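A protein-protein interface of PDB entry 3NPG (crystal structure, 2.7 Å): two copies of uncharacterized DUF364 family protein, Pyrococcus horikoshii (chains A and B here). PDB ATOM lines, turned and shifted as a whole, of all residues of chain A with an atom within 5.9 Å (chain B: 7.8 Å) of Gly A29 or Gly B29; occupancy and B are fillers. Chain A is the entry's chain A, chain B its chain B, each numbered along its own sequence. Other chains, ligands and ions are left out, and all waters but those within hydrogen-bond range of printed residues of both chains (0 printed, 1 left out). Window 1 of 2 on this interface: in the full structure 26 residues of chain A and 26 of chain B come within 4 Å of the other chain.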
ATOM      1  N   SER A  27      18.252 -31.792 -19.672  1.00  0.00           N
ATOM      2  CA  SER A  27      18.323 -30.483 -20.320  1.00  0.00           C
ATOM      3  C   SER A  27      17.361 -29.498 -19.673  1.00  0.00           C
ATOM      4  O   SER A  27      16.155 -29.746 -19.641  1.00  0.00           O
ATOM      5  CB  SER A  27      18.019 -30.601 -21.816  1.00  0.00           C
ATOM      6  OG  SER A  27      18.069 -29.339 -22.459  1.00  0.00           O
ATOM      7  N   PHE A  28      17.889 -28.359 -19.177  1.00  0.00           N
ATOM      8  CA  PHE A  28      17.057 -27.263 -18.694  1.00  0.00           C
ATOM      9  C   PHE A  28      16.649 -26.427 -19.918  1.00  0.00           C
ATOM     10  O   PHE A  28      17.365 -25.506 -20.308  1.00  0.00           O
ATOM     11  CB  PHE A  28      17.826 -26.405 -17.659  1.00  0.00           C
ATOM     12  CG  PHE A  28      17.037 -25.237 -17.104  1.00  0.00           C
ATOM     13  CD1 PHE A  28      16.031 -25.438 -16.167  1.00  0.00           C
ATOM     14  CD2 PHE A  28      17.335 -23.934 -17.480  1.00  0.00           C
ATOM     15  CE1 PHE A  28      15.303 -24.362 -15.660  1.00  0.00           C
ATOM     16  CE2 PHE A  28      16.610 -22.861 -16.970  1.00  0.00           C
ATOM     17  CZ  PHE A  28      15.601 -23.080 -16.062  1.00  0.00           C
ATOM     18  N   GLY A  29      15.605 -26.872 -20.608  1.00  0.00           N
ATOM     19  CA  GLY A  29      15.196 -26.266 -21.867  1.00  0.00           C
ATOM     20  C   GLY A  29      13.750 -25.843 -21.929  1.00  0.00           C
ATOM     21  O   GLY A  29      13.010 -25.997 -20.959  1.00  0.00           O
ATOM     22  N   LEU A  30      13.337 -25.292 -23.095  1.00  0.00           N
ATOM     23  CA  LEU A  30      11.978 -24.808 -23.317  1.00  0.00           C
ATOM     24  C   LEU A  30      11.245 -25.662 -24.378  1.00  0.00           C
ATOM     25  O   LEU A  30      11.860 -26.088 -25.359  1.00  0.00           O
ATOM     26  CB  LEU A  30      11.999 -23.330 -23.753  1.00  0.00           C
ATOM     27  CG  LEU A  30      12.384 -22.310 -22.675  1.00  0.00           C
ATOM     28  CD1 LEU A  30      12.694 -20.974 -23.293  1.00  0.00           C
ATOM     29  CD2 LEU A  30      11.284 -22.163 -21.635  1.00  0.00           C
ATOM     30  N   PRO A  31       9.921 -25.918 -24.205  1.00  0.00           N
ATOM     31  CA  PRO A  31       9.046 -25.453 -23.106  1.00  0.00           C
ATOM     32  C   PRO A  31       9.241 -26.229 -21.802  1.00  0.00           C
ATOM     33  O   PRO A  31       8.851 -25.748 -20.734  1.00  0.00           O
ATOM     34  CB  PRO A  31       7.642 -25.652 -23.688  1.00  0.00           C
ATOM     35  CG  PRO A  31       7.787 -26.828 -24.610  1.00  0.00           C
ATOM     36  CD  PRO A  31       9.167 -26.706 -25.205  1.00  0.00           C
ATOM     37  N   TYR A  32       9.854 -27.423 -21.883  1.00  0.00           N
ATOM     38  CA  TYR A  32      10.004 -28.290 -20.725  1.00  0.00           C
ATOM     39  C   TYR A  32      11.428 -28.678 -20.444  1.00  0.00           C
ATOM     40  O   TYR A  32      12.210 -28.926 -21.373  1.00  0.00           O
ATOM     41  CB  TYR A  32       9.137 -29.549 -20.882  1.00  0.00           C
ATOM     42  CG  TYR A  32       7.672 -29.296 -20.628  1.00  0.00           C
ATOM     43  CD1 TYR A  32       6.845 -28.811 -21.634  1.00  0.00           C
ATOM     44  CD2 TYR A  32       7.116 -29.506 -19.371  1.00  0.00           C
ATOM     45  CE1 TYR A  32       5.509 -28.510 -21.387  1.00  0.00           C
ATOM     46  CE2 TYR A  32       5.776 -29.233 -19.118  1.00  0.00           C
ATOM     47  CZ  TYR A  32       4.975 -28.732 -20.129  1.00  0.00           C
ATOM     48  OH  TYR A  32       3.656 -28.450 -19.886  1.00  0.00           O
ATOM     49  N   THR A  33      11.771 -28.760 -19.146  1.00  0.00           N
ATOM     50  CA  THR A  33      13.018 -29.333 -18.671  1.00  0.00           C
ATOM     51  C   THR A  33      12.781 -30.827 -18.567  1.00  0.00           C
ATOM     52  O   THR A  33      11.709 -31.243 -18.118  1.00  0.00           O
ATOM     53  CB  THR A  33      13.394 -28.728 -17.301  1.00  0.00           C
ATOM     54  OG1 THR A  33      13.668 -27.338 -17.463  1.00  0.00           O
ATOM     55  CG2 THR A  33      14.585 -29.419 -16.659  1.00  0.00           C
ATOM     56  N   TRP A  34      13.714 -31.636 -19.062  1.00  0.00           N
ATOM     57  CA  TRP A  34      13.528 -33.080 -19.046  1.00  0.00           C
ATOM     58  C   TRP A  34      14.702 -33.825 -18.457  1.00  0.00           C
ATOM     59  O   TRP A  34      15.833 -33.344 -18.506  1.00  0.00           O
ATOM     60  CB  TRP A  34      13.186 -33.609 -20.447  1.00  0.00           C
ATOM     61  CG  TRP A  34      14.196 -33.263 -21.492  1.00  0.00           C
ATOM     62  CD1 TRP A  34      14.169 -32.193 -22.336  1.00  0.00           C
ATOM     63  CD2 TRP A  34      15.364 -34.015 -21.833  1.00  0.00           C
ATOM     64  NE1 TRP A  34      15.252 -32.230 -23.182  1.00  0.00           N
ATOM     65  CE2 TRP A  34      15.998 -33.346 -22.903  1.00  0.00           C
ATOM     66  CE3 TRP A  34      15.944 -35.196 -21.335  1.00  0.00           C
ATOM     67  CZ2 TRP A  34      17.187 -33.808 -23.473  1.00  0.00           C
ATOM     68  CZ3 TRP A  34      17.121 -35.649 -21.901  1.00  0.00           C
ATOM     69  CH2 TRP A  34      17.734 -34.955 -22.952  1.00  0.00           C
ATOM     70  N   ALA A  48       9.461 -31.293 -16.446  1.00  0.00           N
ATOM     71  CA  ALA A  48       9.003 -30.253 -15.528  1.00  0.00           C
ATOM     72  C   ALA A  48       9.022 -28.927 -16.251  1.00  0.00           C
ATOM     73  O   ALA A  48      10.046 -28.565 -16.838  1.00  0.00           O
ATOM     74  CB  ALA A  48       9.898 -30.196 -14.301  1.00  0.00           C
ATOM     75  N   THR A  50       9.490 -25.375 -17.586  1.00  0.00           N
ATOM     76  CA  THR A  50      10.458 -24.316 -17.354  1.00  0.00           C
ATOM     77  C   THR A  50       9.727 -22.996 -17.265  1.00  0.00           C
ATOM     78  O   THR A  50       8.880 -22.699 -18.114  1.00  0.00           O
ATOM     79  CB  THR A  50      11.525 -24.316 -18.466  1.00  0.00           C
ATOM     80  OG1 THR A  50      12.095 -25.620 -18.561  1.00  0.00           O
ATOM     81  CG2 THR A  50      12.618 -23.302 -18.218  1.00  0.00           C
ATOM     82  N   LYS A 231      13.552 -31.228 -27.647  1.00  0.00           N
ATOM     83  CA  LYS A 231      14.764 -30.516 -28.061  1.00  0.00           C
ATOM     84  C   LYS A 231      14.449 -29.458 -29.122  1.00  0.00           C
ATOM     85  O   LYS A 231      15.137 -28.438 -29.191  1.00  0.00           O
ATOM     86  CB  LYS A 231      15.817 -31.504 -28.584  1.00  0.00           C
ATOM     87  CG  LYS A 231      16.494 -32.315 -27.494  1.00  0.00           C
ATOM     88  CD  LYS A 231      17.176 -33.546 -28.062  1.00  0.00           C
ATOM     89  CE  LYS A 231      18.034 -34.218 -27.028  1.00  0.00           C
ATOM     90  NZ  LYS A 231      18.335 -35.622 -27.388  1.00  0.00           N
ATOM     91  N   PHE B  26      21.284 -31.428 -30.488  1.00  0.00           N
ATOM     92  CA  PHE B  26      20.801 -30.046 -30.400  1.00  0.00           C
ATOM     93  C   PHE B  26      19.836 -29.898 -29.221  1.00  0.00           C
ATOM     94  O   PHE B  26      19.371 -30.903 -28.675  1.00  0.00           O
ATOM     95  CB  PHE B  26      20.106 -29.624 -31.717  1.00  0.00           C
ATOM     96  CG  PHE B  26      18.862 -30.423 -32.042  1.00  0.00           C
ATOM     97  CD1 PHE B  26      18.951 -31.639 -32.711  1.00  0.00           C
ATOM     98  CD2 PHE B  26      17.604 -29.964 -31.673  1.00  0.00           C
ATOM     99  CE1 PHE B  26      17.805 -32.389 -32.986  1.00  0.00           C
ATOM    100  CE2 PHE B  26      16.460 -30.710 -31.956  1.00  0.00           C
ATOM    101  CZ  PHE B  26      16.568 -31.919 -32.612  1.00  0.00           C
ATOM    102  N   SER B  27      19.505 -28.642 -28.851  1.00  0.00           N
ATOM    103  CA  SER B  27      18.560 -28.365 -27.769  1.00  0.00           C
ATOM    104  C   SER B  27      18.167 -26.905 -27.738  1.00  0.00           C
ATOM    105  O   SER B  27      19.029 -26.034 -27.598  1.00  0.00           O
ATOM    106  CB  SER B  27      19.148 -28.771 -26.413  1.00  0.00           C
ATOM    107  OG  SER B  27      18.247 -28.501 -25.349  1.00  0.00           O
ATOM    108  N   PHE B  28      16.857 -26.628 -27.825  1.00  0.00           N
ATOM    109  CA  PHE B  28      16.335 -25.282 -27.639  1.00  0.00           C
ATOM    110  C   PHE B  28      16.166 -25.062 -26.135  1.00  0.00           C
ATOM    111  O   PHE B  28      15.117 -25.385 -25.573  1.00  0.00           O
ATOM    112  CB  PHE B  28      14.990 -25.109 -28.389  1.00  0.00           C
ATOM    113  CG  PHE B  28      14.369 -23.737 -28.247  1.00  0.00           C
ATOM    114  CD1 PHE B  28      14.892 -22.644 -28.930  1.00  0.00           C
ATOM    115  CD2 PHE B  28      13.234 -23.546 -27.460  1.00  0.00           C
ATOM    116  CE1 PHE B  28      14.326 -21.373 -28.786  1.00  0.00           C
ATOM    117  CE2 PHE B  28      12.661 -22.278 -27.328  1.00  0.00           C
ATOM    118  CZ  PHE B  28      13.208 -21.201 -27.994  1.00  0.00           C
ATOM    119  N   GLY B  29      17.257 -24.676 -25.475  1.00  0.00           N
ATOM    120  CA  GLY B  29      17.285 -24.566 -24.022  1.00  0.00           C
ATOM    121  C   GLY B  29      17.737 -23.230 -23.482  1.00  0.00           C
ATOM    122  O   GLY B  29      18.037 -22.310 -24.247  1.00  0.00           O
ATOM    123  N   LEU B  30      17.787 -23.116 -22.133  1.00  0.00           N
ATOM    124  CA  LEU B  30      18.199 -21.899 -21.442  1.00  0.00           C
ATOM    125  C   LEU B  30      19.523 -22.115 -20.676  1.00  0.00           C
ATOM    126  O   LEU B  30      19.736 -23.191 -20.105  1.00  0.00           O
ATOM    127  CB  LEU B  30      17.099 -21.434 -20.468  1.00  0.00           C
ATOM    128  CG  LEU B  30      15.831 -20.857 -21.102  1.00  0.00           C
ATOM    129  CD1 LEU B  30      14.740 -20.753 -20.091  1.00  0.00           C
ATOM    130  CD2 LEU B  30      16.094 -19.496 -21.727  1.00  0.00           C
ATOM    131  N   PRO B  31      20.431 -21.094 -20.638  1.00  0.00           N
ATOM    132  CA  PRO B  31      20.300 -19.751 -21.241  1.00  0.00           C
ATOM    133  C   PRO B  31      20.538 -19.741 -22.753  1.00  0.00           C
ATOM    134  O   PRO B  31      20.148 -18.788 -23.429  1.00  0.00           O
ATOM    135  CB  PRO B  31      21.362 -18.940 -20.487  1.00  0.00           C
ATOM    136  CG  PRO B  31      22.429 -19.942 -20.161  1.00  0.00           C
ATOM    137  CD  PRO B  31      21.701 -21.234 -19.888  1.00  0.00           C
ATOM    138  N   TYR B  32      21.163 -20.808 -23.287  1.00  0.00           N
ATOM    139  CA  TYR B  32      21.528 -20.862 -24.692  1.00  0.00           C
ATOM    140  C   TYR B  32      20.981 -22.066 -25.413  1.00  0.00           C
ATOM    141  O   TYR B  32      20.936 -23.163 -24.855  1.00  0.00           O
ATOM    142  CB  TYR B  32      23.063 -20.797 -24.853  1.00  0.00           C
ATOM    143  CG  TYR B  32      23.626 -19.409 -24.648  1.00  0.00           C
ATOM    144  CD1 TYR B  32      23.910 -18.931 -23.373  1.00  0.00           C
ATOM    145  CD2 TYR B  32      23.839 -18.557 -25.726  1.00  0.00           C
ATOM    146  CE1 TYR B  32      24.369 -17.632 -23.173  1.00  0.00           C
ATOM    147  CE2 TYR B  32      24.323 -17.263 -25.541  1.00  0.00           C
ATOM    148  CZ  TYR B  32      24.590 -16.804 -24.260  1.00  0.00           C
ATOM    149  OH  TYR B  32      25.066 -15.531 -24.065  1.00  0.00           O
ATOM    150  N   THR B  33      20.588 -21.865 -26.679  1.00  0.00           N
ATOM    151  CA  THR B  33      20.210 -22.928 -27.599  1.00  0.00           C
ATOM    152  C   THR B  33      21.485 -23.369 -28.318  1.00  0.00           C
ATOM    153  O   THR B  33      22.228 -22.518 -28.825  1.00  0.00           O
ATOM    154  CB  THR B  33      19.143 -22.417 -28.584  1.00  0.00           C
ATOM    155  OG1 THR B  33      17.911 -22.246 -27.886  1.00  0.00           O
ATOM    156  CG2 THR B  33      18.941 -23.353 -29.776  1.00  0.00           C
ATOM    157  N   TRP B  34      21.785 -24.678 -28.299  1.00  0.00           N
ATOM    158  CA  TRP B  34      23.035 -25.173 -28.857  1.00  0.00           C
ATOM    159  C   TRP B  34      22.846 -26.222 -29.947  1.00  0.00           C
ATOM    160  O   TRP B  34      21.846 -26.935 -29.961  1.00  0.00           O
ATOM    161  CB  TRP B  34      23.953 -25.698 -27.744  1.00  0.00           C
ATOM    162  CG  TRP B  34      23.334 -26.766 -26.896  1.00  0.00           C
ATOM    163  CD1 TRP B  34      22.681 -26.597 -25.709  1.00  0.00           C
ATOM    164  CD2 TRP B  34      23.354 -28.176 -27.149  1.00  0.00           C
ATOM    165  NE1 TRP B  34      22.288 -27.817 -25.209  1.00  0.00           N
ATOM    166  CE2 TRP B  34      22.693 -28.806 -26.071  1.00  0.00           C
ATOM    167  CE3 TRP B  34      23.866 -28.974 -28.188  1.00  0.00           C
ATOM    168  CZ2 TRP B  34      22.514 -30.196 -26.010  1.00  0.00           C
ATOM    169  CZ3 TRP B  34      23.702 -30.350 -28.118  1.00  0.00           C
ATOM    170  CH2 TRP B  34      23.030 -30.947 -27.041  1.00  0.00           C
ATOM    171  N   ALA B  48      23.352 -20.064 -29.524  1.00  0.00           N
ATOM    172  CA  ALA B  48      22.566 -18.862 -29.799  1.00  0.00           C
ATOM    173  C   ALA B  48      21.721 -18.560 -28.572  1.00  0.00           C
ATOM    174  O   ALA B  48      21.199 -19.484 -27.951  1.00  0.00           O
ATOM    175  CB  ALA B  48      21.670 -19.083 -31.008  1.00  0.00           C
ATOM    176  N   MET B  49      21.642 -17.286 -28.170  1.00  0.00           N
ATOM    177  CA  MET B  49      20.894 -16.924 -26.969  1.00  0.00           C
ATOM    178  C   MET B  49      19.397 -17.112 -27.139  1.00  0.00           C
ATOM    179  O   MET B  49      18.799 -16.563 -28.072  1.00  0.00           O
ATOM    180  CB  MET B  49      21.211 -15.497 -26.522  1.00  0.00           C
ATOM    181  CG  MET B  49      20.676 -15.183 -25.138  1.00  0.00           C
ATOM    182  SD  MET B  49      20.954 -13.363 -24.630  1.00  0.00           S
ATOM    183  CE  MET B  49      19.655 -13.255 -23.181  1.00  0.00           C
ATOM    184  N   THR B  50      18.785 -17.886 -26.228  1.00  0.00           N
ATOM    185  CA  THR B  50      17.345 -18.079 -26.219  1.00  0.00           C
ATOM    186  C   THR B  50      16.674 -16.858 -25.590  1.00  0.00           C
ATOM    187  O   THR B  50      17.108 -16.384 -24.525  1.00  0.00           O
ATOM    188  CB  THR B  50      16.974 -19.390 -25.492  1.00  0.00           C
ATOM    189  OG1 THR B  50      17.643 -20.480 -26.126  1.00  0.00           O
ATOM    190  CG2 THR B  50      15.476 -19.648 -25.483  1.00  0.00           C
ATOM    191  N   LEU B  51      15.663 -16.307 -26.280  1.00  0.00           N
ATOM    192  CA  LEU B  51      14.902 -15.156 -25.796  1.00  0.00           C
ATOM    193  C   LEU B  51      13.439 -15.591 -25.559  1.00  0.00           C
ATOM    194  O   LEU B  51      12.610 -15.525 -26.472  1.00  0.00           O
ATOM    195  CB  LEU B  51      14.978 -13.987 -26.808  1.00  0.00           C
ATOM    196  CG  LEU B  51      16.399 -13.555 -27.236  1.00  0.00           C
ATOM    197  CD1 LEU B  51      16.357 -12.694 -28.465  1.00  0.00           C
ATOM    198  CD2 LEU B  51      17.130 -12.842 -26.103  1.00  0.00           C
ATOM    199  N   PRO B  52      13.145 -16.167 -24.363  1.00  0.00           N
ATOM    200  CA  PRO B  52      11.789 -16.695 -24.113  1.00  0.00           C
ATOM    201  C   PRO B  52      10.680 -15.645 -24.200  1.00  0.00           C
ATOM    202  O   PRO B  52       9.556 -15.971 -24.582  1.00  0.00           O
ATOM    203  CB  PRO B  52      11.896 -17.295 -22.707  1.00  0.00           C
ATOM    204  CG  PRO B  52      13.082 -16.637 -22.097  1.00  0.00           C
ATOM    205  CD  PRO B  52      14.030 -16.383 -23.202  1.00  0.00           C
ATOM    206  N   TYR B  58       4.976 -22.526 -28.738  1.00  0.00           N
ATOM    207  CA  TYR B  58       5.995 -23.570 -28.705  1.00  0.00           C
ATOM    208  C   TYR B  58       5.745 -24.592 -29.791  1.00  0.00           C
ATOM    209  O   TYR B  58       5.235 -25.687 -29.528  1.00  0.00           O
ATOM    210  CB  TYR B  58       6.104 -24.214 -27.309  1.00  0.00           C
ATOM    211  CG  TYR B  58       6.814 -23.326 -26.310  1.00  0.00           C
ATOM    212  CD1 TYR B  58       8.199 -23.170 -26.347  1.00  0.00           C
ATOM    213  CD2 TYR B  58       6.100 -22.581 -25.378  1.00  0.00           C
ATOM    214  CE1 TYR B  58       8.854 -22.319 -25.459  1.00  0.00           C
ATOM    215  CE2 TYR B  58       6.744 -21.725 -24.487  1.00  0.00           C
ATOM    216  CZ  TYR B  58       8.123 -21.596 -24.532  1.00  0.00           C
ATOM    217  OH  TYR B  58       8.764 -20.767 -23.650  1.00  0.00           O
ATOM    218  N   THR B  83      16.514 -19.356 -33.631  1.00  0.00           N
ATOM    219  CA  THR B  83      17.541 -19.617 -32.614  1.00  0.00           C
ATOM    220  C   THR B  83      18.299 -20.918 -32.911  1.00  0.00           C
ATOM    221  O   THR B  83      19.530 -20.927 -32.884  1.00  0.00           O
ATOM    222  CB  THR B  83      16.929 -19.572 -31.196  1.00  0.00           C
ATOM    223  OG1 THR B  83      16.068 -18.437 -31.095  1.00  0.00           O
ATOM    224  CG2 THR B  83      17.978 -19.498 -30.120  1.00  0.00           C
ATOM    225  N   LEU B  84      17.565 -21.995 -33.283  1.00  0.00           N
ATOM    226  CA  LEU B  84      18.179 -23.276 -33.667  1.00  0.00           C
ATOM    227  C   LEU B  84      18.998 -23.135 -34.962  1.00  0.00           C
ATOM    228  O   LEU B  84      20.030 -23.784 -35.110  1.00  0.00           O
ATOM    229  CB  LEU B  84      17.104 -24.367 -33.831  1.00  0.00           C
ATOM    230  CG  LEU B  84      16.602 -25.020 -32.533  1.00  0.00           C
ATOM    231  CD1 LEU B  84      15.243 -25.648 -32.733  1.00  0.00           C
ATOM    232  CD2 LEU B  84      17.575 -26.052 -32.034  1.00  0.00           C
ATOM    233  N   LEU B 230      25.753 -26.262 -20.200  1.00  0.00           N
ATOM    234  CA  LEU B 230      24.651 -25.705 -20.998  1.00  0.00           C
ATOM    235  C   LEU B 230      23.335 -26.393 -20.622  1.00  0.00           C
ATOM    236  O   LEU B 230      22.310 -25.730 -20.478  1.00  0.00           O
ATOM    237  CB  LEU B 230      24.923 -25.881 -22.507  1.00  0.00           C
ATOM    238  CG  LEU B 230      25.877 -24.871 -23.151  1.00  0.00           C
ATOM    239  CD1 LEU B 230      26.233 -25.291 -24.545  1.00  0.00           C
ATOM    240  CD2 LEU B 230      25.270 -23.478 -23.179  1.00  0.00           C
ATOM    241  N   LYS B 231      23.377 -27.723 -20.429  1.00  0.00           N
ATOM    242  CA  LYS B 231      22.210 -28.514 -20.028  1.00  0.00           C
ATOM    243  C   LYS B 231      21.786 -28.191 -18.578  1.00  0.00           C
ATOM    244  O   LYS B 231      20.608 -28.309 -18.241  1.00  0.00           O
ATOM    245  CB  LYS B 231      22.502 -30.021 -20.182  1.00  0.00           C
ATOM    246  CG  LYS B 231      22.528 -30.497 -21.624  1.00  0.00           C
ATOM    247  CD  LYS B 231      23.235 -31.832 -21.758  1.00  0.00           C
ATOM    248  CE  LYS B 231      23.065 -32.404 -23.138  1.00  0.00           C
ATOM    249  NZ  LYS B 231      24.076 -33.433 -23.438  1.00  0.00           N
ATOM    250  N   LEU B 232      22.755 -27.781 -17.725  1.00  0.00           N
ATOM    251  CA  LEU B 232      22.482 -27.423 -16.326  1.00  0.00           C
ATOM    252  C   LEU B 232      21.970 -25.988 -16.187  1.00  0.00           C
ATOM    253  O   LEU B 232      21.494 -25.606 -15.116  1.00  0.00           O
ATOM    254  CB  LEU B 232      23.728 -27.635 -15.445  1.00  0.00           C
ATOM    255  CG  LEU B 232      23.987 -29.076 -14.980  1.00  0.00           C
ATOM    256  CD1 LEU B 232      25.402 -29.235 -14.470  1.00  0.00           C
ATOM    257  CD2 LEU B 232      22.990 -29.502 -13.912  1.00  0.00           C
ATOM    258  N   GLY B 233      22.066 -25.212 -17.270  1.00  0.00           N
ATOM    259  CA  GLY B 233      21.590 -23.834 -17.294  1.00  0.00           C
ATOM    260  C   GLY B 233      22.533 -22.847 -16.633  1.00  0.00           C
ATOM    261  O   GLY B 233      22.092 -21.818 -16.115  1.00  0.00           O
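The side-chain hydroxyl of Ser A27 is in hydrogen-bond range of the side-chain hydroxyl of Ser B27, 3.0 Å away.
The backbone carbonyl oxygen (O) of Phe A28 lies within hydrogen-bond range of the backbone NH (N) of Leu B30, at 3.0 Å.
The backbone NH (N) of Phe A28 is in hydrogen-bond range of the backbone carbonyl oxygen (O) of Lys B231.
O of Phe B28 lies within hydrogen-bond range of N of Leu A30, at 3.1 Å.
The backbone carbonyl oxygen of Lys A231 is in hydrogen-bond range of the backbone NH of Phe B28 (2.8 Å).
The backbone carbonyl oxygen (O) of Gly A29 sits at hydrogen-bond distance from the side-chain hydroxyl (OG1) of Thr A50 (2.6 Å).
The backbone carbonyl oxygen (O) of Pro A31 lies within hydrogen-bond range of the backbone NH (N) of Thr A50, 3.2 Å away.
OG1 of Thr A33 lies within hydrogen-bond range of OG1 of Thr A50, 2.6 Å away.
N of Gly B29 sits at hydrogen-bond distance from OG1 of Thr B33 (3.5 Å).
The backbone carbonyl oxygen of Pro B31 is in hydrogen-bond range of the backbone NH of Thr B50 (3.2 Å).
The side-chain hydroxyl (OG1) of Thr B50 is in hydrogen-bond range of the side-chain hydroxyl (OG1) of Thr B33.
Among the printed residues, merely in contact across the chains: Lys A231 with Phe B26, Gly A29 with Gly B29, Leu A30 with Tyr B58, Pro A31 with Tyr B58, Lys A231 with Ser B27, Ser A27 with Lys B231, Leu A30 with Thr B50, Leu A30 with Leu B30, Thr A50 with Leu B30, Leu A30 with Pro B52, Gly A29 with Phe B28 and Phe A28 with Gly B29.
Of the printed residues of chain B, Leu A30 touches Phe B28, Leu B30, Thr B50, Pro B52 and Tyr B58.
Of the printed residues of chain B, Thr A50 touches Leu B30.
Printed residues of chain A within 4 Å of Ser B27: Ser A27 and Lys A231.
Gly B29 touches just these residues of chain A: Phe A28 and Gly A29.
Of the printed residues of chain A, Pro B52 touches Leu A30 (3.8 Å).
The nearest residue of chain B that does not touch Gly A29 is Leu B30 (4.1 Å).
The nearest printed residue of chain A that does not touch Ser B27 is Gly A29 (5.1 Å).
Hydrophobic or aromatic side chains of chain A within 4 Å of the printed part of chain B: Phe A28, Leu A30 and Pro A31.
Of the 21 printed residues of chain B, 9 touch a printed residue of chain A.
Printed residues of chain B that touch a printed residue of chain A: Phe B26, Ser B27, Phe B28, Gly B29, Leu B30, Thr B50, Pro B52, Tyr B58 and Lys B231.
Among the printed residues, 17 pairs touch across the chains.
Among the printed residues, no Asp or Glu carboxylate lies within 4 Å of a Lys or Arg side-chain nitrogen of the other chain.
Ser A27 touches its own counterpart, Ser B27.
Ser A27 touches Lys B231, and with the chains exchanged Lys A231 touches Ser B27.
Gly B29 touches its own counterpart, Gly A29.
Leu B30 touches its own counterpart, Leu A30.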
